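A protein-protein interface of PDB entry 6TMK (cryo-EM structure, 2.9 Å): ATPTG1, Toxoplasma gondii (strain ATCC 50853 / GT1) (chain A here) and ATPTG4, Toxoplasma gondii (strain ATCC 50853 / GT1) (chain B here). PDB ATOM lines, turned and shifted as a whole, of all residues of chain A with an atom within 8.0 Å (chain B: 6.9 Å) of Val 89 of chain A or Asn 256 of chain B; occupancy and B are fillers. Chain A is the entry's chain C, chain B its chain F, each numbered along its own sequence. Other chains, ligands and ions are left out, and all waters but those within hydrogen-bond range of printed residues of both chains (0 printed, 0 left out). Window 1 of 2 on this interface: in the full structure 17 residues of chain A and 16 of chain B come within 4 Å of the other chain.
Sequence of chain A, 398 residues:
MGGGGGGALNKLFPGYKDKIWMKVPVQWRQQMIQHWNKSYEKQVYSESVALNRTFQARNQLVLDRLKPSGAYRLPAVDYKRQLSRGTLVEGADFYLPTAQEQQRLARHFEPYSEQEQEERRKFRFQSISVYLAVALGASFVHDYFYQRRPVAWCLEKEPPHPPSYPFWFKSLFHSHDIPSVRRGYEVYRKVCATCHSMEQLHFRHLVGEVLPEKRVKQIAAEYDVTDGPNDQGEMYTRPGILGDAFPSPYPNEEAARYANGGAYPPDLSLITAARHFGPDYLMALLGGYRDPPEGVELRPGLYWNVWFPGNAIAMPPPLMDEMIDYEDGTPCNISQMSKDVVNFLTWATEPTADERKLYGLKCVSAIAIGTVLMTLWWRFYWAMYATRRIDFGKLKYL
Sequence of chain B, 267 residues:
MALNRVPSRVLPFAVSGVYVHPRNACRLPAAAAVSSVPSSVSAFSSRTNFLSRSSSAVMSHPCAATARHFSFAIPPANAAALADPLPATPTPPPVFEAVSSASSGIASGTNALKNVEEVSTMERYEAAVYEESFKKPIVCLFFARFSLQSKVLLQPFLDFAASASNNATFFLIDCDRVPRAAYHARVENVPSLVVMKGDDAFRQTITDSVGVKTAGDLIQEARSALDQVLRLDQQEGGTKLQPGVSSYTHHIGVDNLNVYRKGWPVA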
ATOM      1  N   ALA A  76       0.086  15.452   2.224  1.00  0.00           N
ATOM      2  CA  ALA A  76      -0.473  15.899   3.489  1.00  0.00           C
ATOM      3  C   ALA A  76      -0.184  17.383   3.652  1.00  0.00           C
ATOM      4  O   ALA A  76       0.621  17.968   2.923  1.00  0.00           O
ATOM      5  CB  ALA A  76       0.101  15.099   4.656  1.00  0.00           C
ATOM      6  N   VAL A  77      -0.852  17.979   4.634  1.00  0.00           N
ATOM      7  CA  VAL A  77      -0.722  19.390   4.959  1.00  0.00           C
ATOM      8  C   VAL A  77      -0.443  19.506   6.448  1.00  0.00           C
ATOM      9  O   VAL A  77      -0.972  18.730   7.249  1.00  0.00           O
ATOM     10  CB  VAL A  77      -1.990  20.179   4.572  1.00  0.00           C
ATOM     11  CG1 VAL A  77      -1.884  21.617   5.008  1.00  0.00           C
ATOM     12  CG2 VAL A  77      -2.231  20.101   3.090  1.00  0.00           C
ATOM     13  N   ASP A  78       0.390  20.472   6.819  1.00  0.00           N
ATOM     14  CA  ASP A  78       0.822  20.579   8.201  1.00  0.00           C
ATOM     15  C   ASP A  78      -0.349  20.895   9.126  1.00  0.00           C
ATOM     16  O   ASP A  78      -1.346  21.512   8.735  1.00  0.00           O
ATOM     17  CB  ASP A  78       1.911  21.641   8.334  1.00  0.00           C
ATOM     18  CG  ASP A  78       1.493  22.979   7.779  1.00  0.00           C
ATOM     19  OD1 ASP A  78       1.060  23.845   8.568  1.00  0.00           O
ATOM     20  OD2 ASP A  78       1.599  23.166   6.551  1.00  0.00           O
ATOM     21  N   TYR A  79      -0.210  20.449  10.376  1.00  0.00           N
ATOM     22  CA  TYR A  79      -1.313  20.527  11.321  1.00  0.00           C
ATOM     23  C   TYR A  79      -1.651  21.964  11.673  1.00  0.00           C
ATOM     24  O   TYR A  79      -2.814  22.271  11.945  1.00  0.00           O
ATOM     25  CB  TYR A  79      -0.981  19.710  12.572  1.00  0.00           C
ATOM     26  CG  TYR A  79      -0.032  20.362  13.548  1.00  0.00           C
ATOM     27  CD1 TYR A  79      -0.501  20.959  14.704  1.00  0.00           C
ATOM     28  CD2 TYR A  79       1.333  20.362  13.325  1.00  0.00           C
ATOM     29  CE1 TYR A  79       0.358  21.545  15.599  1.00  0.00           C
ATOM     30  CE2 TYR A  79       2.199  20.946  14.215  1.00  0.00           C
ATOM     31  CZ  TYR A  79       1.706  21.536  15.352  1.00  0.00           C
ATOM     32  OH  TYR A  79       2.565  22.125  16.250  1.00  0.00           O
ATOM     33  N   GLN A  82      -3.807  23.185   8.789  1.00  0.00           N
ATOM     34  CA  GLN A  82      -5.138  22.598   8.928  1.00  0.00           C
ATOM     35  C   GLN A  82      -5.926  23.262  10.050  1.00  0.00           C
ATOM     36  O   GLN A  82      -7.128  23.521   9.910  1.00  0.00           O
ATOM     37  CB  GLN A  82      -5.043  21.099   9.178  1.00  0.00           C
ATOM     38  CG  GLN A  82      -4.741  20.275   7.967  1.00  0.00           C
ATOM     39  CD  GLN A  82      -4.405  18.857   8.316  1.00  0.00           C
ATOM     40  OE1 GLN A  82      -4.276  18.506   9.485  1.00  0.00           O
ATOM     41  NE2 GLN A  82      -4.284  18.019   7.303  1.00  0.00           N
ATOM     42  N   LEU A  83      -5.268  23.542  11.172  1.00  0.00           N
ATOM     43  CA  LEU A  83      -5.939  24.185  12.292  1.00  0.00           C
ATOM     44  C   LEU A  83      -6.426  25.573  11.914  1.00  0.00           C
ATOM     45  O   LEU A  83      -7.494  26.008  12.359  1.00  0.00           O
ATOM     46  CB  LEU A  83      -4.987  24.262  13.478  1.00  0.00           C
ATOM     47  CG  LEU A  83      -5.593  24.572  14.838  1.00  0.00           C
ATOM     48  CD1 LEU A  83      -6.398  23.397  15.331  1.00  0.00           C
ATOM     49  CD2 LEU A  83      -4.504  24.915  15.811  1.00  0.00           C
ATOM     50  N   GLY A  86      -9.486  25.251   9.788  1.00  0.00           N
ATOM     51  CA  GLY A  86     -10.637  24.662  10.437  1.00  0.00           C
ATOM     52  C   GLY A  86     -10.918  23.243  10.009  1.00  0.00           C
ATOM     53  O   GLY A  86     -12.078  22.826   9.972  1.00  0.00           O
ATOM     54  N   THR A  87      -9.874  22.487   9.688  1.00  0.00           N
ATOM     55  CA  THR A  87      -9.985  21.191   9.043  1.00  0.00           C
ATOM     56  C   THR A  87      -9.497  20.039   9.904  1.00  0.00           C
ATOM     57  O   THR A  87      -9.844  18.889   9.620  1.00  0.00           O
ATOM     58  CB  THR A  87      -9.215  21.194   7.713  1.00  0.00           C
ATOM     59  OG1 THR A  87      -9.820  22.127   6.815  1.00  0.00           O
ATOM     60  CG2 THR A  87      -9.213  19.843   7.082  1.00  0.00           C
ATOM     61  N   LEU A  88      -8.727  20.313  10.949  1.00  0.00           N
ATOM     62  CA  LEU A  88      -8.034  19.269  11.681  1.00  0.00           C
ATOM     63  C   LEU A  88      -9.004  18.408  12.478  1.00  0.00           C
ATOM     64  O   LEU A  88      -9.930  18.909  13.121  1.00  0.00           O
ATOM     65  CB  LEU A  88      -7.002  19.896  12.608  1.00  0.00           C
ATOM     66  CG  LEU A  88      -6.050  18.967  13.340  1.00  0.00           C
ATOM     67  CD1 LEU A  88      -4.975  18.489  12.408  1.00  0.00           C
ATOM     68  CD2 LEU A  88      -5.445  19.707  14.483  1.00  0.00           C
ATOM     69  N   VAL A  89      -8.775  17.100  12.427  1.00  0.00           N
ATOM     70  CA  VAL A  89      -9.431  16.124  13.281  1.00  0.00           C
ATOM     71  C   VAL A  89      -8.354  15.378  14.052  1.00  0.00           C
ATOM     72  O   VAL A  89      -7.304  15.035  13.500  1.00  0.00           O
ATOM     73  CB  VAL A  89     -10.305  15.147  12.467  1.00  0.00           C
ATOM     74  CG1 VAL A  89     -10.970  14.147  13.371  1.00  0.00           C
ATOM     75  CG2 VAL A  89     -11.340  15.899  11.694  1.00  0.00           C
ATOM     76  N   GLU A  90      -8.620  15.135  15.334  1.00  0.00           N
ATOM     77  CA  GLU A  90      -7.632  14.588  16.251  1.00  0.00           C
ATOM     78  C   GLU A  90      -7.833  13.117  16.587  1.00  0.00           C
ATOM     79  O   GLU A  90      -6.881  12.475  17.038  1.00  0.00           O
ATOM     80  CB  GLU A  90      -7.645  15.381  17.561  1.00  0.00           C
ATOM     81  CG  GLU A  90      -7.198  16.817  17.437  1.00  0.00           C
ATOM     82  CD  GLU A  90      -8.339  17.801  17.558  1.00  0.00           C
ATOM     83  OE1 GLU A  90      -9.441  17.505  17.055  1.00  0.00           O
ATOM     84  OE2 GLU A  90      -8.132  18.877  18.156  1.00  0.00           O
ATOM     85  N   GLY A  91      -9.027  12.565  16.376  1.00  0.00           N
ATOM     86  CA  GLY A  91      -9.471  11.391  17.092  1.00  0.00           C
ATOM     87  C   GLY A  91      -9.248  10.080  16.354  1.00  0.00           C
ATOM     88  O   GLY A  91      -8.698  10.016  15.259  1.00  0.00           O
ATOM     89  N   ALA A  92      -9.718   9.011  16.998  1.00  0.00           N
ATOM     90  CA  ALA A  92      -9.771   7.669  16.425  1.00  0.00           C
ATOM     91  C   ALA A  92      -8.372   7.153  16.074  1.00  0.00           C
ATOM     92  O   ALA A  92      -7.983   7.020  14.914  1.00  0.00           O
ATOM     93  CB  ALA A  92     -10.688   7.646  15.195  1.00  0.00           C
ATOM     94  N   ARG B 180     -12.890  23.525   0.305  1.00  0.00           N
ATOM     95  CA  ARG B 180     -12.492  22.128   0.369  1.00  0.00           C
ATOM     96  C   ARG B 180     -12.102  21.583  -0.995  1.00  0.00           C
ATOM     97  O   ARG B 180     -11.331  20.621  -1.071  1.00  0.00           O
ATOM     98  CB  ARG B 180     -13.621  21.304   0.969  1.00  0.00           C
ATOM     99  CG  ARG B 180     -13.618  21.278   2.472  1.00  0.00           C
ATOM    100  CD  ARG B 180     -14.499  20.175   2.995  1.00  0.00           C
ATOM    101  NE  ARG B 180     -13.878  18.871   2.812  1.00  0.00           N
ATOM    102  CZ  ARG B 180     -14.544  17.727   2.776  1.00  0.00           C
ATOM    103  NH1 ARG B 180     -13.892  16.595   2.597  1.00  0.00           N
ATOM    104  NH2 ARG B 180     -15.858  17.712   2.920  1.00  0.00           N
ATOM    105  N   HIS B 251      -7.126  11.452   0.801  1.00  0.00           N
ATOM    106  CA  HIS B 251      -6.912  12.875   1.039  1.00  0.00           C
ATOM    107  C   HIS B 251      -7.191  13.243   2.490  1.00  0.00           C
ATOM    108  O   HIS B 251      -7.755  14.298   2.784  1.00  0.00           O
ATOM    109  CB  HIS B 251      -7.758  13.710   0.085  1.00  0.00           C
ATOM    110  CG  HIS B 251      -7.579  13.336  -1.349  1.00  0.00           C
ATOM    111  ND1 HIS B 251      -6.442  13.651  -2.059  1.00  0.00           N
ATOM    112  CD2 HIS B 251      -8.377  12.652  -2.199  1.00  0.00           C
ATOM    113  CE1 HIS B 251      -6.553  13.188  -3.290  1.00  0.00           C
ATOM    114  NE2 HIS B 251      -7.719  12.577  -3.400  1.00  0.00           N
ATOM    115  N   ILE B 252      -6.785  12.370   3.404  1.00  0.00           N
ATOM    116  CA  ILE B 252      -7.020  12.605   4.819  1.00  0.00           C
ATOM    117  C   ILE B 252      -5.915  13.455   5.435  1.00  0.00           C
ATOM    118  O   ILE B 252      -6.178  14.239   6.351  1.00  0.00           O
ATOM    119  CB  ILE B 252      -7.183  11.273   5.563  1.00  0.00           C
ATOM    120  CG1 ILE B 252      -8.541  10.668   5.235  1.00  0.00           C
ATOM    121  CG2 ILE B 252      -7.039  11.473   7.047  1.00  0.00           C
ATOM    122  CD1 ILE B 252      -8.652   9.219   5.538  1.00  0.00           C
ATOM    123  N   GLY B 253      -4.678  13.313   4.959  1.00  0.00           N
ATOM    124  CA  GLY B 253      -3.620  14.191   5.417  1.00  0.00           C
ATOM    125  C   GLY B 253      -3.772  15.589   4.868  1.00  0.00           C
ATOM    126  O   GLY B 253      -3.319  16.557   5.484  1.00  0.00           O
ATOM    127  N   VAL B 254      -4.407  15.712   3.710  1.00  0.00           N
ATOM    128  CA  VAL B 254      -4.661  17.009   3.106  1.00  0.00           C
ATOM    129  C   VAL B 254      -5.843  17.686   3.780  1.00  0.00           C
ATOM    130  O   VAL B 254      -5.787  18.869   4.131  1.00  0.00           O
ATOM    131  CB  VAL B 254      -4.899  16.835   1.598  1.00  0.00           C
ATOM    132  CG1 VAL B 254      -5.365  18.122   0.976  1.00  0.00           C
ATOM    133  CG2 VAL B 254      -3.652  16.329   0.928  1.00  0.00           C
ATOM    134  N   ASP B 255      -6.923  16.940   3.977  1.00  0.00           N
ATOM    135  CA  ASP B 255      -8.134  17.441   4.614  1.00  0.00           C
ATOM    136  C   ASP B 255      -8.673  16.335   5.507  1.00  0.00           C
ATOM    137  O   ASP B 255      -9.227  15.351   5.009  1.00  0.00           O
ATOM    138  CB  ASP B 255      -9.169  17.857   3.574  1.00  0.00           C
ATOM    139  CG  ASP B 255     -10.234  18.768   4.139  1.00  0.00           C
ATOM    140  OD1 ASP B 255     -10.077  20.000   4.036  1.00  0.00           O
ATOM    141  OD2 ASP B 255     -11.228  18.255   4.688  1.00  0.00           O
ATOM    142  N   ASN B 256      -8.506  16.492   6.820  1.00  0.00           N
ATOM    143  CA  ASN B 256      -8.867  15.435   7.752  1.00  0.00           C
ATOM    144  C   ASN B 256     -10.358  15.146   7.768  1.00  0.00           C
ATOM    145  O   ASN B 256     -10.764  14.127   8.334  1.00  0.00           O
ATOM    146  CB  ASN B 256      -8.427  15.789   9.172  1.00  0.00           C
ATOM    147  CG  ASN B 256      -6.937  15.967   9.304  1.00  0.00           C
ATOM    148  OD1 ASN B 256      -6.467  16.989   9.788  1.00  0.00           O
ATOM    149  ND2 ASN B 256      -6.187  14.968   8.894  1.00  0.00           N
ATOM    150  N   LEU B 257     -11.181  16.003   7.172  1.00  0.00           N
ATOM    151  CA  LEU B 257     -12.621  15.803   7.211  1.00  0.00           C
ATOM    152  C   LEU B 257     -13.087  14.655   6.335  1.00  0.00           C
ATOM    153  O   LEU B 257     -14.279  14.334   6.355  1.00  0.00           O
ATOM    154  CB  LEU B 257     -13.336  17.085   6.797  1.00  0.00           C
ATOM    155  CG  LEU B 257     -13.002  18.330   7.617  1.00  0.00           C
ATOM    156  CD1 LEU B 257     -13.722  19.536   7.068  1.00  0.00           C
ATOM    157  CD2 LEU B 257     -13.346  18.130   9.071  1.00  0.00           C
ATOM    158  N   ASN B 258     -12.195  14.029   5.570  1.00  0.00           N
ATOM    159  CA  ASN B 258     -12.572  12.867   4.780  1.00  0.00           C
ATOM    160  C   ASN B 258     -12.755  11.616   5.626  1.00  0.00           C
ATOM    161  O   ASN B 258     -13.270  10.615   5.117  1.00  0.00           O
ATOM    162  CB  ASN B 258     -11.530  12.615   3.698  1.00  0.00           C
ATOM    163  CG  ASN B 258     -11.520  13.687   2.637  1.00  0.00           C
ATOM    164  OD1 ASN B 258     -12.379  13.715   1.760  1.00  0.00           O
ATOM    165  ND2 ASN B 258     -10.552  14.581   2.712  1.00  0.00           N
ATOM    166  N   VAL B 259     -12.350  11.643   6.897  1.00  0.00           N
ATOM    167  CA  VAL B 259     -12.616  10.513   7.776  1.00  0.00           C
ATOM    168  C   VAL B 259     -14.113  10.320   7.947  1.00  0.00           C
ATOM    169  O   VAL B 259     -14.594   9.188   8.061  1.00  0.00           O
ATOM    170  CB  VAL B 259     -11.921  10.713   9.136  1.00  0.00           C
ATOM    171  CG1 VAL B 259     -10.444  10.885   8.954  1.00  0.00           C
ATOM    172  CG2 VAL B 259     -12.496  11.906   9.856  1.00  0.00           C
ATOM    173  N   TYR B 260     -14.873  11.415   7.966  1.00  0.00           N
ATOM    174  CA  TYR B 260     -16.324  11.301   8.036  1.00  0.00           C
ATOM    175  C   TYR B 260     -16.878  10.632   6.790  1.00  0.00           C
ATOM    176  O   TYR B 260     -17.738   9.749   6.877  1.00  0.00           O
ATOM    177  CB  TYR B 260     -16.946  12.680   8.213  1.00  0.00           C
ATOM    178  CG  TYR B 260     -16.639  13.336   9.528  1.00  0.00           C
ATOM    179  CD1 TYR B 260     -17.302  12.963  10.681  1.00  0.00           C
ATOM    180  CD2 TYR B 260     -15.694  14.338   9.616  1.00  0.00           C
ATOM    181  CE1 TYR B 260     -17.022  13.565  11.883  1.00  0.00           C
ATOM    182  CE2 TYR B 260     -15.411  14.944  10.812  1.00  0.00           C
ATOM    183  CZ  TYR B 260     -16.078  14.556  11.941  1.00  0.00           C
ATOM    184  OH  TYR B 260     -15.791  15.164  13.135  1.00  0.00           O
ATOM    185  N   PRO B 265     -14.425   6.414  12.905  1.00  0.00           N
ATOM    186  CA  PRO B 265     -14.792   7.134  14.124  1.00  0.00           C
ATOM    187  C   PRO B 265     -13.927   8.368  14.313  1.00  0.00           C
ATOM    188  O   PRO B 265     -12.908   8.566  13.652  1.00  0.00           O
ATOM    189  CB  PRO B 265     -14.567   6.101  15.229  1.00  0.00           C
ATOM    190  CG  PRO B 265     -13.592   5.150  14.675  1.00  0.00           C
ATOM    191  CD  PRO B 265     -13.818   5.108  13.200  1.00  0.00           C
ATOM    192  N   VAL B 266     -14.371   9.225  15.227  1.00  0.00           N
ATOM    193  CA  VAL B 266     -13.607  10.405  15.607  1.00  0.00           C
ATOM    194  C   VAL B 266     -13.577  10.517  17.124  1.00  0.00           C
ATOM    195  O   VAL B 266     -13.076  11.502  17.676  1.00  0.00           O
ATOM    196  CB  VAL B 266     -14.199  11.673  14.976  1.00  0.00           C
ATOM    197  CG1 VAL B 266     -13.861  11.725  13.508  1.00  0.00           C
ATOM    198  CG2 VAL B 266     -15.697  11.713  15.183  1.00  0.00           C
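O of Gly 253 of chain B lies within hydrogen-bond range of N of Val 77 of chain A (3.0 Å).
OE1 of Gln 82 of chain A sits close to OD1 of Asn 256 of chain B, at 2.7 Å.
O of Gly 253 of chain B sits at hydrogen-bond distance from NE2 of Gln 82 of chain A (2.5 Å).
N of Leu 257 of chain B sits close to OD2 of Asp 255 of chain B (3.4 Å).
The backbone carbonyl oxygen of Asp 255 of chain B is in hydrogen-bond range of the side-chain amide nitrogen of Asn 258 of chain B.
The guanidinium group (NE) of Arg 180 of chain B lies within salt-bridge range of the side-chain carboxylate (OD2) of Asp 255 of chain B.
O of Ile 252 of chain B is in hydrogen-bond range of ND2 of Asn 256 of chain B (2.6 Å).
NE2 of Gln 82 of chain A lies within hydrogen-bond range of O of Val 77 of chain A.
O of Gln 82 of chain A sits at hydrogen-bond distance from N of Thr 87 of chain A, at 2.9 Å.
Among the printed residues, pairs that only touch across the chains: Ala 92 of chain A with Pro 265 of chain B (2.9 Å), Thr 87 of chain A with Asp 255 of chain B (3.2 Å), Leu 88 of chain A with Asn 256 of chain B (3.4 Å), Thr 87 of chain A with Asn 256 of chain B (3.4 Å), Val 89 of chain A with Asn 256 of chain B (3.5 Å), Ala 76 of chain A with Gly 253 of chain B (3.5 Å), Gln 82 of chain A with Val 254 of chain B (3.6 Å), Thr 87 of chain A with Leu 257 of chain B (3.6 Å), Gly 91 of chain A with Val 266 of chain B (3.7 Å), Val 89 of chain A with Val 266 of chain B (3.8 Å), Val 77 of chain A with Val 254 of chain B (3.9 Å), Ala 76 of chain A with Val 254 of chain B (3.9 Å) and Val 89 of chain A with Leu 257 of chain B (3.99 Å).
Of the printed residues of chain B, Val 89 of chain A touches Asn 256 (3.5 Å), Leu 257 (3.99 Å) and Val 266 (3.8 Å).
Asn 256 of chain B touches just these residues of chain A: Gln 82, Thr 87, Leu 88 and Val 89.
Printed residues of chain A within 4 Å of Leu 257 of chain B: Thr 87 (3.6 Å) and Val 89 (3.99 Å).
Of the printed residues of chain A, Pro 265 of chain B touches Ala 92 (2.9 Å).
Printed residues of chain B within 4 Å of Gln 82 of chain A: Gly 253 (2.5 Å), Val 254 (3.6 Å) and Asn 256 (2.7 Å).
The nearest printed residue of chain B that does not touch Gly 91 of chain A is Pro 265 of chain B (4.7 Å).
Of the 13 printed residues of chain B, 7 touch a printed residue of chain A.
Printed residues of chain B that touch a printed residue of chain A: Gly 253, Val 254, Asp 255, Asn 256, Leu 257, Pro 265 and Val 266.
Hydrophobic or aromatic side chains of chain B that line the printed part of chain A: Leu 257, Pro 265 and Val 266.
Along chain B the printed residues that touch a printed residue of chain A span positions 253 to 266.
Hydrophobic or aromatic side chains of chain A that line the printed part of chain B: Ala 76, Val 77, Leu 88, Val 89 and Ala 92.
Among the printed residues, 16 pairs touch across the chains.
Among the printed residues, no Asp or Glu carboxylate lies within 4 Å of a Lys or Arg side-chain nitrogen of the other chain.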
